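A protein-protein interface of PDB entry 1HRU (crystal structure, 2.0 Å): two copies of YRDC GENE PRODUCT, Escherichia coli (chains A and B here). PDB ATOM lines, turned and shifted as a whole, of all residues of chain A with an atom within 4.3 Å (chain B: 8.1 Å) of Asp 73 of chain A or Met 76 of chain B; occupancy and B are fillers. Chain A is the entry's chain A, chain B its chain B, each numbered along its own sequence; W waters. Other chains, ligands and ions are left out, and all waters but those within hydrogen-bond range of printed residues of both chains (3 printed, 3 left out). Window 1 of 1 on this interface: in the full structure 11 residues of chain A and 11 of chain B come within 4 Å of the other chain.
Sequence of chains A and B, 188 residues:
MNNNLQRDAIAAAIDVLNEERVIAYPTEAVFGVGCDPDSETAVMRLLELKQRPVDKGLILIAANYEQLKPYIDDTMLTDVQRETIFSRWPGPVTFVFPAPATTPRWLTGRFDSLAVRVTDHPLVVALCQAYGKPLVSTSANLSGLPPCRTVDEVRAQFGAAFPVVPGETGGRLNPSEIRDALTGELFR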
ATOM      1  N   ILE A  72      -1.877 -28.243 -24.528  1.00  0.00           N
ATOM      2  CA  ILE A  72      -0.912 -27.277 -24.016  1.00  0.00           C
ATOM      3  C   ILE A  72       0.523 -27.763 -24.080  1.00  0.00           C
ATOM      4  O   ILE A  72       0.793 -28.928 -24.379  1.00  0.00           O
ATOM      5  CB  ILE A  72      -1.215 -26.924 -22.541  1.00  0.00           C
ATOM      6  CG1 ILE A  72      -1.203 -28.203 -21.693  1.00  0.00           C
ATOM      7  CG2 ILE A  72      -2.573 -26.231 -22.415  1.00  0.00           C
ATOM      8  CD1 ILE A  72      -1.432 -27.955 -20.199  1.00  0.00           C
ATOM      9  N   ASP A  73       1.442 -26.847 -23.804  1.00  0.00           N
ATOM     10  CA  ASP A  73       2.868 -27.151 -23.774  1.00  0.00           C
ATOM     11  C   ASP A  73       3.390 -26.761 -22.395  1.00  0.00           C
ATOM     12  O   ASP A  73       3.455 -25.571 -22.072  1.00  0.00           O
ATOM     13  CB  ASP A  73       3.606 -26.338 -24.836  1.00  0.00           C
ATOM     14  CG  ASP A  73       5.112 -26.533 -24.779  1.00  0.00           C
ATOM     15  OD1 ASP A  73       5.812 -25.937 -25.624  1.00  0.00           O
ATOM     16  OD2 ASP A  73       5.594 -27.280 -23.897  1.00  0.00           O
ATOM     17  N   ASP A  74       3.741 -27.750 -21.575  1.00  0.00           N
ATOM     18  CA  ASP A  74       4.259 -27.465 -20.230  1.00  0.00           C
ATOM     19  C   ASP A  74       5.714 -27.900 -20.109  1.00  0.00           C
ATOM     20  O   ASP A  74       6.261 -27.957 -19.008  1.00  0.00           O
ATOM     21  CB  ASP A  74       3.433 -28.205 -19.176  1.00  0.00           C
ATOM     22  CG  ASP A  74       3.578 -29.715 -19.273  1.00  0.00           C
ATOM     23  OD1 ASP A  74       2.906 -30.447 -18.516  1.00  0.00           O
ATOM     24  OD2 ASP A  74       4.366 -30.180 -20.116  1.00  0.00           O
ATOM     25  N   THR A  75       6.355 -28.192 -21.237  1.00  0.00           N
ATOM     26  CA  THR A  75       7.730 -28.668 -21.193  1.00  0.00           C
ATOM     27  C   THR A  75       8.775 -27.725 -20.614  1.00  0.00           C
ATOM     28  O   THR A  75       9.846 -28.178 -20.214  1.00  0.00           O
ATOM     29  CB  THR A  75       8.220 -29.119 -22.590  1.00  0.00           C
ATOM     30  OG1 THR A  75       8.221 -28.002 -23.486  1.00  0.00           O
ATOM     31  CG2 THR A  75       7.314 -30.206 -23.137  1.00  0.00           C
ATOM     32  N   MET A  76       8.464 -26.429 -20.548  1.00  0.00           N
ATOM     33  CA  MET A  76       9.398 -25.424 -20.037  1.00  0.00           C
ATOM     34  C   MET A  76       9.308 -25.202 -18.519  1.00  0.00           C
ATOM     35  O   MET A  76      10.196 -24.582 -17.914  1.00  0.00           O
ATOM     36  CB  MET A  76       9.157 -24.074 -20.739  1.00  0.00           C
ATOM     37  CG  MET A  76       7.855 -23.333 -20.340  1.00  0.00           C
ATOM     38  SD  MET A  76       6.271 -24.075 -20.920  1.00  0.00           S
ATOM     39  CE  MET A  76       6.472 -23.969 -22.791  1.00  0.00           C
ATOM     40  N   PRO A  98       1.429 -21.946 -22.374  1.00  0.00           N
ATOM     41  CA  PRO A  98       1.725 -21.725 -23.788  1.00  0.00           C
ATOM     42  C   PRO A  98       1.059 -22.914 -24.484  1.00  0.00           C
ATOM     43  O   PRO A  98       0.823 -23.953 -23.849  1.00  0.00           O
ATOM     44  CB  PRO A  98       3.257 -21.781 -23.846  1.00  0.00           C
ATOM     45  CG  PRO A  98       3.680 -22.318 -22.528  1.00  0.00           C
ATOM     46  CD  PRO A  98       2.650 -21.852 -21.559  1.00  0.00           C
ATOM     47  N   ALA A  99       0.735 -22.782 -25.761  1.00  0.00           N
ATOM     48  CA  ALA A  99       0.089 -23.890 -26.451  1.00  0.00           C
ATOM     49  C   ALA A  99       0.800 -24.197 -27.755  1.00  0.00           C
ATOM     50  O   ALA A  99       1.210 -23.288 -28.483  1.00  0.00           O
ATOM     51  CB  ALA A  99      -1.388 -23.568 -26.715  1.00  0.00           C
ATOM     52  N   PRO A 100       0.958 -25.488 -28.071  1.00  0.00           N
ATOM     53  CA  PRO A 100       1.642 -25.790 -29.326  1.00  0.00           C
ATOM     54  C   PRO A 100       0.823 -25.269 -30.502  1.00  0.00           C
ATOM     55  O   PRO A 100      -0.399 -25.066 -30.382  1.00  0.00           O
ATOM     56  CB  PRO A 100       1.791 -27.322 -29.291  1.00  0.00           C
ATOM     57  CG  PRO A 100       0.628 -27.779 -28.440  1.00  0.00           C
ATOM     58  CD  PRO A 100       0.519 -26.712 -27.368  1.00  0.00           C
ATOM     59  N   ALA A 101       1.500 -25.029 -31.622  1.00  0.00           N
ATOM     60  CA  ALA A 101       0.854 -24.527 -32.824  1.00  0.00           C
ATOM     61  C   ALA A 101      -0.121 -25.564 -33.368  1.00  0.00           C
ATOM     62  O   ALA A 101      -0.911 -25.271 -34.259  1.00  0.00           O
ATOM     63  CB  ALA A 101       1.899 -24.179 -33.881  1.00  0.00           C
ATOM     64  N   ASP A 112      -0.618 -17.628 -28.544  1.00  0.00           N
ATOM     65  CA  ASP A 112       0.121 -18.889 -28.567  1.00  0.00           C
ATOM     66  C   ASP A 112      -0.003 -19.500 -27.167  1.00  0.00           C
ATOM     67  O   ASP A 112       0.935 -20.082 -26.644  1.00  0.00           O
ATOM     68  CB  ASP A 112       1.606 -18.660 -28.904  1.00  0.00           C
ATOM     69  CG  ASP A 112       1.837 -18.392 -30.382  1.00  0.00           C
ATOM     70  OD1 ASP A 112       2.989 -18.092 -30.764  1.00  0.00           O
ATOM     71  OD2 ASP A 112       0.867 -18.485 -31.168  1.00  0.00           O
ATOM     72  N   ILE B  72      16.019 -25.548 -27.241  1.00  0.00           N
ATOM     73  CA  ILE B  72      14.868 -24.656 -27.202  1.00  0.00           C
ATOM     74  C   ILE B  72      13.541 -25.345 -27.512  1.00  0.00           C
ATOM     75  O   ILE B  72      13.504 -26.522 -27.907  1.00  0.00           O
ATOM     76  CB  ILE B  72      15.071 -23.497 -28.191  1.00  0.00           C
ATOM     77  CG1 ILE B  72      15.281 -24.060 -29.600  1.00  0.00           C
ATOM     78  CG2 ILE B  72      16.279 -22.652 -27.758  1.00  0.00           C
ATOM     79  CD1 ILE B  72      15.438 -23.011 -30.680  1.00  0.00           C
ATOM     80  N   ASP B  73      12.451 -24.614 -27.292  1.00  0.00           N
ATOM     81  CA  ASP B  73      11.105 -25.118 -27.578  1.00  0.00           C
ATOM     82  C   ASP B  73      10.432 -24.090 -28.478  1.00  0.00           C
ATOM     83  O   ASP B  73      10.086 -22.987 -28.029  1.00  0.00           O
ATOM     84  CB  ASP B  73      10.313 -25.275 -26.276  1.00  0.00           C
ATOM     85  CG  ASP B  73       8.847 -25.605 -26.512  1.00  0.00           C
ATOM     86  OD1 ASP B  73       8.106 -25.695 -25.514  1.00  0.00           O
ATOM     87  OD2 ASP B  73       8.421 -25.770 -27.681  1.00  0.00           O
ATOM     88  N   ASP B  74      10.270 -24.438 -29.751  1.00  0.00           N
ATOM     89  CA  ASP B  74       9.635 -23.550 -30.719  1.00  0.00           C
ATOM     90  C   ASP B  74       8.277 -24.115 -31.132  1.00  0.00           C
ATOM     91  O   ASP B  74       7.690 -23.630 -32.087  1.00  0.00           O
ATOM     92  CB  ASP B  74      10.507 -23.419 -31.976  1.00  0.00           C
ATOM     93  CG  ASP B  74      10.551 -24.715 -32.798  1.00  0.00           C
ATOM     94  OD1 ASP B  74      11.318 -24.784 -33.783  1.00  0.00           O
ATOM     95  OD2 ASP B  74       9.818 -25.672 -32.456  1.00  0.00           O
ATOM     96  N   THR B  75       7.775 -25.123 -30.413  1.00  0.00           N
ATOM     97  CA  THR B  75       6.501 -25.749 -30.784  1.00  0.00           C
ATOM     98  C   THR B  75       5.258 -24.860 -30.741  1.00  0.00           C
ATOM     99  O   THR B  75       4.254 -25.166 -31.399  1.00  0.00           O
ATOM    100  CB  THR B  75       6.190 -27.016 -29.939  1.00  0.00           C
ATOM    101  OG1 THR B  75       5.938 -26.642 -28.579  1.00  0.00           O
ATOM    102  CG2 THR B  75       7.354 -28.040 -30.021  1.00  0.00           C
ATOM    103  N   MET B  76       5.311 -23.772 -29.977  1.00  0.00           N
ATOM    104  CA  MET B  76       4.172 -22.862 -29.880  1.00  0.00           C
ATOM    105  C   MET B  76       4.120 -21.885 -31.062  1.00  0.00           C
ATOM    106  O   MET B  76       3.071 -21.287 -31.335  1.00  0.00           O
ATOM    107  CB  MET B  76       4.232 -22.055 -28.571  1.00  0.00           C
ATOM    108  CG  MET B  76       5.324 -20.969 -28.494  1.00  0.00           C
ATOM    109  SD  MET B  76       7.063 -21.599 -28.305  1.00  0.00           S
ATOM    110  CE  MET B  76       6.935 -22.465 -26.695  1.00  0.00           C
ATOM    111  N   LEU B  77       5.244 -21.733 -31.760  1.00  0.00           N
ATOM    112  CA  LEU B  77       5.340 -20.793 -32.879  1.00  0.00           C
ATOM    113  C   LEU B  77       4.665 -21.269 -34.149  1.00  0.00           C
ATOM    114  O   LEU B  77       4.966 -22.346 -34.669  1.00  0.00           O
ATOM    115  CB  LEU B  77       6.809 -20.470 -33.178  1.00  0.00           C
ATOM    116  CG  LEU B  77       7.599 -19.817 -32.047  1.00  0.00           C
ATOM    117  CD1 LEU B  77       9.087 -19.763 -32.411  1.00  0.00           C
ATOM    118  CD2 LEU B  77       7.049 -18.435 -31.787  1.00  0.00           C
ATOM    119  N   THR B  78       3.750 -20.447 -34.651  1.00  0.00           N
ATOM    120  CA  THR B  78       3.002 -20.761 -35.865  1.00  0.00           C
ATOM    121  C   THR B  78       3.965 -20.650 -37.044  1.00  0.00           C
ATOM    122  O   THR B  78       5.051 -20.073 -36.916  1.00  0.00           O
ATOM    123  CB  THR B  78       1.842 -19.765 -36.069  1.00  0.00           C
ATOM    124  OG1 THR B  78       2.370 -18.443 -36.265  1.00  0.00           O
ATOM    125  CG2 THR B  78       0.955 -19.725 -34.821  1.00  0.00           C
ATOM    126  N   ASP B  79       3.577 -21.204 -38.190  1.00  0.00           N
ATOM    127  CA  ASP B  79       4.436 -21.124 -39.367  1.00  0.00           C
ATOM    128  C   ASP B  79       4.704 -19.685 -39.805  1.00  0.00           C
ATOM    129  O   ASP B  79       5.790 -19.381 -40.314  1.00  0.00           O
ATOM    130  CB  ASP B  79       3.844 -21.938 -40.523  1.00  0.00           C
ATOM    131  CG  ASP B  79       4.095 -23.426 -40.360  1.00  0.00           C
ATOM    132  OD1 ASP B  79       5.004 -23.789 -39.579  1.00  0.00           O
ATOM    133  OD2 ASP B  79       3.405 -24.231 -41.014  1.00  0.00           O
ATOM    134  N   GLN B  81       4.844 -17.047 -37.737  1.00  0.00           N
ATOM    135  CA  GLN B  81       5.777 -16.472 -36.768  1.00  0.00           C
ATOM    136  C   GLN B  81       7.187 -16.968 -37.075  1.00  0.00           C
ATOM    137  O   GLN B  81       8.160 -16.219 -36.986  1.00  0.00           O
ATOM    138  CB  GLN B  81       5.398 -16.868 -35.331  1.00  0.00           C
ATOM    139  CG  GLN B  81       4.061 -16.257 -34.851  1.00  0.00           C
ATOM    140  CD  GLN B  81       3.682 -16.666 -33.432  1.00  0.00           C
ATOM    141  OE1 GLN B  81       3.511 -17.853 -33.130  1.00  0.00           O
ATOM    142  NE2 GLN B  81       3.542 -15.679 -32.554  1.00  0.00           N
ATOM    143  N   ARG B  82       7.300 -18.238 -37.443  1.00  0.00           N
ATOM    144  CA  ARG B  82       8.604 -18.812 -37.753  1.00  0.00           C
ATOM    145  C   ARG B  82       9.251 -18.135 -38.951  1.00  0.00           C
ATOM    146  O   ARG B  82      10.448 -17.830 -38.950  1.00  0.00           O
ATOM    147  CB  ARG B  82       8.464 -20.313 -38.014  1.00  0.00           C
ATOM    148  CG  ARG B  82       8.073 -21.069 -36.763  1.00  0.00           C
ATOM    149  CD  ARG B  82       8.127 -22.567 -36.950  1.00  0.00           C
ATOM    150  NE  ARG B  82       7.534 -23.248 -35.800  1.00  0.00           N
ATOM    151  CZ  ARG B  82       7.691 -24.542 -35.532  1.00  0.00           C
ATOM    152  NH1 ARG B  82       8.433 -25.301 -36.330  1.00  0.00           N
ATOM    153  NH2 ARG B  82       7.089 -25.081 -34.482  1.00  0.00           N
ATOM    154  N   VAL B  96      15.328 -14.876 -28.245  1.00  0.00           N
ATOM    155  CA  VAL B  96      15.077 -15.553 -26.982  1.00  0.00           C
ATOM    156  C   VAL B  96      13.881 -16.471 -27.216  1.00  0.00           C
ATOM    157  O   VAL B  96      12.818 -16.009 -27.614  1.00  0.00           O
ATOM    158  CB  VAL B  96      14.740 -14.533 -25.868  1.00  0.00           C
ATOM    159  CG1 VAL B  96      14.315 -15.256 -24.602  1.00  0.00           C
ATOM    160  CG2 VAL B  96      15.950 -13.658 -25.585  1.00  0.00           C
ATOM    161  N   PHE B  97      14.075 -17.771 -26.998  1.00  0.00           N
ATOM    162  CA  PHE B  97      13.035 -18.792 -27.186  1.00  0.00           C
ATOM    163  C   PHE B  97      12.708 -19.451 -25.854  1.00  0.00           C
ATOM    164  O   PHE B  97      13.551 -19.505 -24.958  1.00  0.00           O
ATOM    165  CB  PHE B  97      13.537 -19.942 -28.071  1.00  0.00           C
ATOM    166  CG  PHE B  97      13.561 -19.647 -29.537  1.00  0.00           C
ATOM    167  CD1 PHE B  97      12.592 -20.196 -30.378  1.00  0.00           C
ATOM    168  CD2 PHE B  97      14.547 -18.846 -30.085  1.00  0.00           C
ATOM    169  CE1 PHE B  97      12.609 -19.950 -31.740  1.00  0.00           C
ATOM    170  CE2 PHE B  97      14.574 -18.593 -31.452  1.00  0.00           C
ATOM    171  CZ  PHE B  97      13.605 -19.145 -32.280  1.00  0.00           C
ATOM    172  N   PRO B  98      11.479 -19.963 -25.704  1.00  0.00           N
ATOM    173  CA  PRO B  98      11.166 -20.626 -24.440  1.00  0.00           C
ATOM    174  C   PRO B  98      12.144 -21.801 -24.454  1.00  0.00           C
ATOM    175  O   PRO B  98      12.638 -22.174 -25.522  1.00  0.00           O
ATOM    176  CB  PRO B  98       9.736 -21.095 -24.650  1.00  0.00           C
ATOM    177  CG  PRO B  98       9.154 -20.006 -25.496  1.00  0.00           C
ATOM    178  CD  PRO B  98      10.261 -19.744 -26.505  1.00  0.00           C
ATOM    179  N   ALA B  99      12.429 -22.390 -23.301  1.00  0.00           N
ATOM    180  CA  ALA B  99      13.350 -23.514 -23.275  1.00  0.00           C
ATOM    181  C   ALA B  99      12.779 -24.634 -22.426  1.00  0.00           C
ATOM    182  O   ALA B  99      12.217 -24.394 -21.358  1.00  0.00           O
ATOM    183  CB  ALA B  99      14.704 -23.075 -22.720  1.00  0.00           C
ATOM    184  N   PRO B 100      12.925 -25.878 -22.883  1.00  0.00           N
ATOM    185  CA  PRO B 100      12.407 -27.013 -22.115  1.00  0.00           C
ATOM    186  C   PRO B 100      13.117 -27.039 -20.764  1.00  0.00           C
ATOM    187  O   PRO B 100      14.240 -26.526 -20.641  1.00  0.00           O
ATOM    188  CB  PRO B 100      12.810 -28.235 -22.956  1.00  0.00           C
ATOM    189  CG  PRO B 100      13.204 -27.674 -24.295  1.00  0.00           C
ATOM    190  CD  PRO B 100      13.771 -26.328 -24.002  1.00  0.00           C
ATOM    191  N   ALA B 101      12.479 -27.643 -19.766  1.00  0.00           N
ATOM    192  CA  ALA B 101      13.082 -27.765 -18.444  1.00  0.00           C
ATOM    193  C   ALA B 101      14.291 -28.691 -18.528  1.00  0.00           C
ATOM    194  O   ALA B 101      15.103 -28.753 -17.604  1.00  0.00           O
ATOM    195  CB  ALA B 101      12.068 -28.324 -17.441  1.00  0.00           C
ATOM    196  N   ASP B 112      12.926 -19.533 -18.114  1.00  0.00           N
ATOM    197  CA  ASP B 112      12.473 -20.728 -18.812  1.00  0.00           C
ATOM    198  C   ASP B 112      12.641 -20.393 -20.275  1.00  0.00           C
ATOM    199  O   ASP B 112      11.791 -20.724 -21.105  1.00  0.00           O
ATOM    200  CB  ASP B 112      10.994 -21.030 -18.524  1.00  0.00           C
ATOM    201  CG  ASP B 112      10.767 -21.600 -17.133  1.00  0.00           C
ATOM    202  OD1 ASP B 112       9.595 -21.869 -16.785  1.00  0.00           O
ATOM    203  OD2 ASP B 112      11.750 -21.777 -16.385  1.00  0.00           O
ATOM    204  N   ALA B 181      11.341 -14.234 -29.387  1.00  0.00           N
ATOM    205  CA  ALA B 181      10.791 -15.030 -30.478  1.00  0.00           C
ATOM    206  C   ALA B 181       9.262 -14.993 -30.543  1.00  0.00           C
ATOM    207  O   ALA B 181       8.679 -15.065 -31.621  1.00  0.00           O
ATOM    208  CB  ALA B 181      11.264 -16.473 -30.348  1.00  0.00           C
ATOM    209  N   LEU B 182       8.623 -14.890 -29.383  1.00  0.00           N
ATOM    210  CA  LEU B 182       7.167 -14.880 -29.298  1.00  0.00           C
ATOM    211  C   LEU B 182       6.536 -13.550 -29.685  1.00  0.00           C
ATOM    212  O   LEU B 182       5.383 -13.508 -30.107  1.00  0.00           O
ATOM    213  CB  LEU B 182       6.729 -15.247 -27.878  1.00  0.00           C
ATOM    214  CG  LEU B 182       7.281 -16.578 -27.357  1.00  0.00           C
ATOM    215  CD1 LEU B 182       6.872 -16.779 -25.907  1.00  0.00           C
ATOM    216  CD2 LEU B 182       6.767 -17.714 -28.222  1.00  0.00           C
HETATM  217  O   HOH W   1       4.888 -28.880 -27.272  1.00  0.00           O
HETATM  218  O   HOH W   2       3.326 -15.133 -29.659  1.00  0.00           O
HETATM  219  O   HOH W   3      11.002 -30.569 -20.087  1.00  0.00           O
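OD1 of Asp 73 of chain A touches CE of Met 76 of chain B, at 3.8 Å.
CE of Met 76 of chain A touches OD1 of Asp 73 of chain B, at 3.6 Å.
CA of Met 76 of chain A touches CA of Pro 100 of chain B, at 3.99 Å.
Met 76 of chain A touches Ala 101 of chain B (CA to N, 3.8 Å).
Ala 99 of chain A touches Met 76 of chain B.
Pro 100 of chain A touches Thr 75 of chain B.
CA of Pro 100 of chain A touches CA of Met 76 of chain B (3.9 Å).
Ala 101 of chain A touches Met 76 of chain B.
Ala 101 of chain A touches Leu 77 of chain B.
Thr 78 of chain B touches Asp 112 of chain A.
Asp 73 of chain A touches Met 76 of chain B, and with the chains exchanged Met 76 of chain A touches Asp 73 of chain B.
Thr 75 of chain A touches Ala 101 of chain B, and with the chains exchanged Ala 101 of chain A touches Thr 75 of chain B.
Met 76 of chain A touches Pro 100 of chain B, and with the chains exchanged Pro 100 of chain A touches Met 76 of chain B.
Met 76 of chain A touches Ala 101 of chain B, and with the chains exchanged Ala 101 of chain A touches Met 76 of chain B.
Positions printed for both chains: 72, 73, 74, 75, 76, 98, 99, 100, 101 and 112.
Asp 73 of chain A touches three residues of chain B.
Met 76 of chain B touches just these residues of chain A: Asp 73, Ala 99, Pro 100, Ala 101 and Asp 112.
Of the printed residues of chain A, Leu 77 of chain B touches Ala 101.
Printed residues of chain B within 4 Å of Met 76 of chain A: Asp 73, Ala 99, Pro 100, Ala 101 and Asp 112.
Printed residues of chain A within 4 Å of Gln 81 of chain B: Asp 112.
Printed residues of chain B within 4 Å of Ala 99 of chain A: Met 76.
Leu 182 of chain B touches none of the printed residues of chain A.
Ile 72 of chain A touches none of the printed residues of chain B.
The backbone carbonyl oxygen (O) of Pro 98 of chain B lies within hydrogen-bond range of the backbone NH (N) of Asp 73 of chain B (3.0 Å).
The side-chain amide oxygen (OE1) of Gln 81 of chain B lies within hydrogen-bond range of the backbone NH (N) of Thr 78 of chain B, at 3.0 Å.
OG1 of Thr 75 of chain B sits at hydrogen-bond distance from OD2 of Asp 73 of chain B.
The side-chain carboxylate (OD2) of Asp 73 of chain A sits at hydrogen-bond distance from the side-chain hydroxyl (OG1) of Thr 75 of chain A, at 2.8 Å.
O of Asp 112 of chain B is in hydrogen-bond range of N of Ala 99 of chain B (2.8 Å).
NE of Arg 82 of chain B is in hydrogen-bond range of O of Leu 77 of chain B (2.9 Å).
Water W3 lies within hydrogen-bond range of O of Thr 75 of chain A (2.7 Å) and N of Ala 101 of chain B (3.3 Å).
Water W2 lies within hydrogen-bond range of the backbone carbonyl oxygen of Leu 182 of chain B (2.7 Å), the side-chain amide nitrogen of Gln 81 of chain B (3.0 Å) and the side-chain carboxylate of Asp 112 of chain A (3.2 Å).
Water W1 lies within hydrogen-bond range of the side-chain hydroxyl (OG1) of Thr 75 of chain B (2.8 Å) and the side-chain carboxylate (OD1) of Asp 73 of chain A (3.5 Å).
N of Ala 101 of chain B is in hydrogen-bond range of O of Thr 75 of chain A, at 2.7 Å.
The backbone carbonyl oxygen (O) of Met 76 of chain B lies close to the side-chain carboxylate (OD1) of Asp 112 of chain A (3.2 Å).
O of Met 76 of chain A sits close to OD1 of Asp 112 of chain B, 3.0 Å away.
The side-chain amide oxygen (OE1) of Gln 81 of chain B lies close to the side-chain carboxylate (OD1) of Asp 112 of chain A.
N of Ala 101 of chain A sits at hydrogen-bond distance from O of Thr 75 of chain B (2.8 Å).
OD1 of Asp 73 of chain A sits at hydrogen-bond distance from OG1 of Thr 75 of chain B (3.0 Å).
The side-chain hydroxyl (OG1) of Thr 75 of chain A sits at hydrogen-bond distance from the side-chain carboxylate (OD1) of Asp 73 of chain B.
The side-chain carboxylate (OD1) of Asp 73 of chain A lies close to the side-chain carboxylate (OD1) of Asp 73 of chain B, at 2.3 Å.
Of the 19 printed residues of chain B, 10 touch a printed residue of chain A.
Hydrophobic or aromatic side chains of chain B that line the printed part of chain A: Met 76 and Ala 101.
Hydrophobic or aromatic side chains of chain A that line the printed part of chain B: Met 76, Pro 100 and Ala 101.
Among the printed residues, no Asp or Glu carboxylate lies within 4 Å of a Lys or Arg side-chain nitrogen of the other chain.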
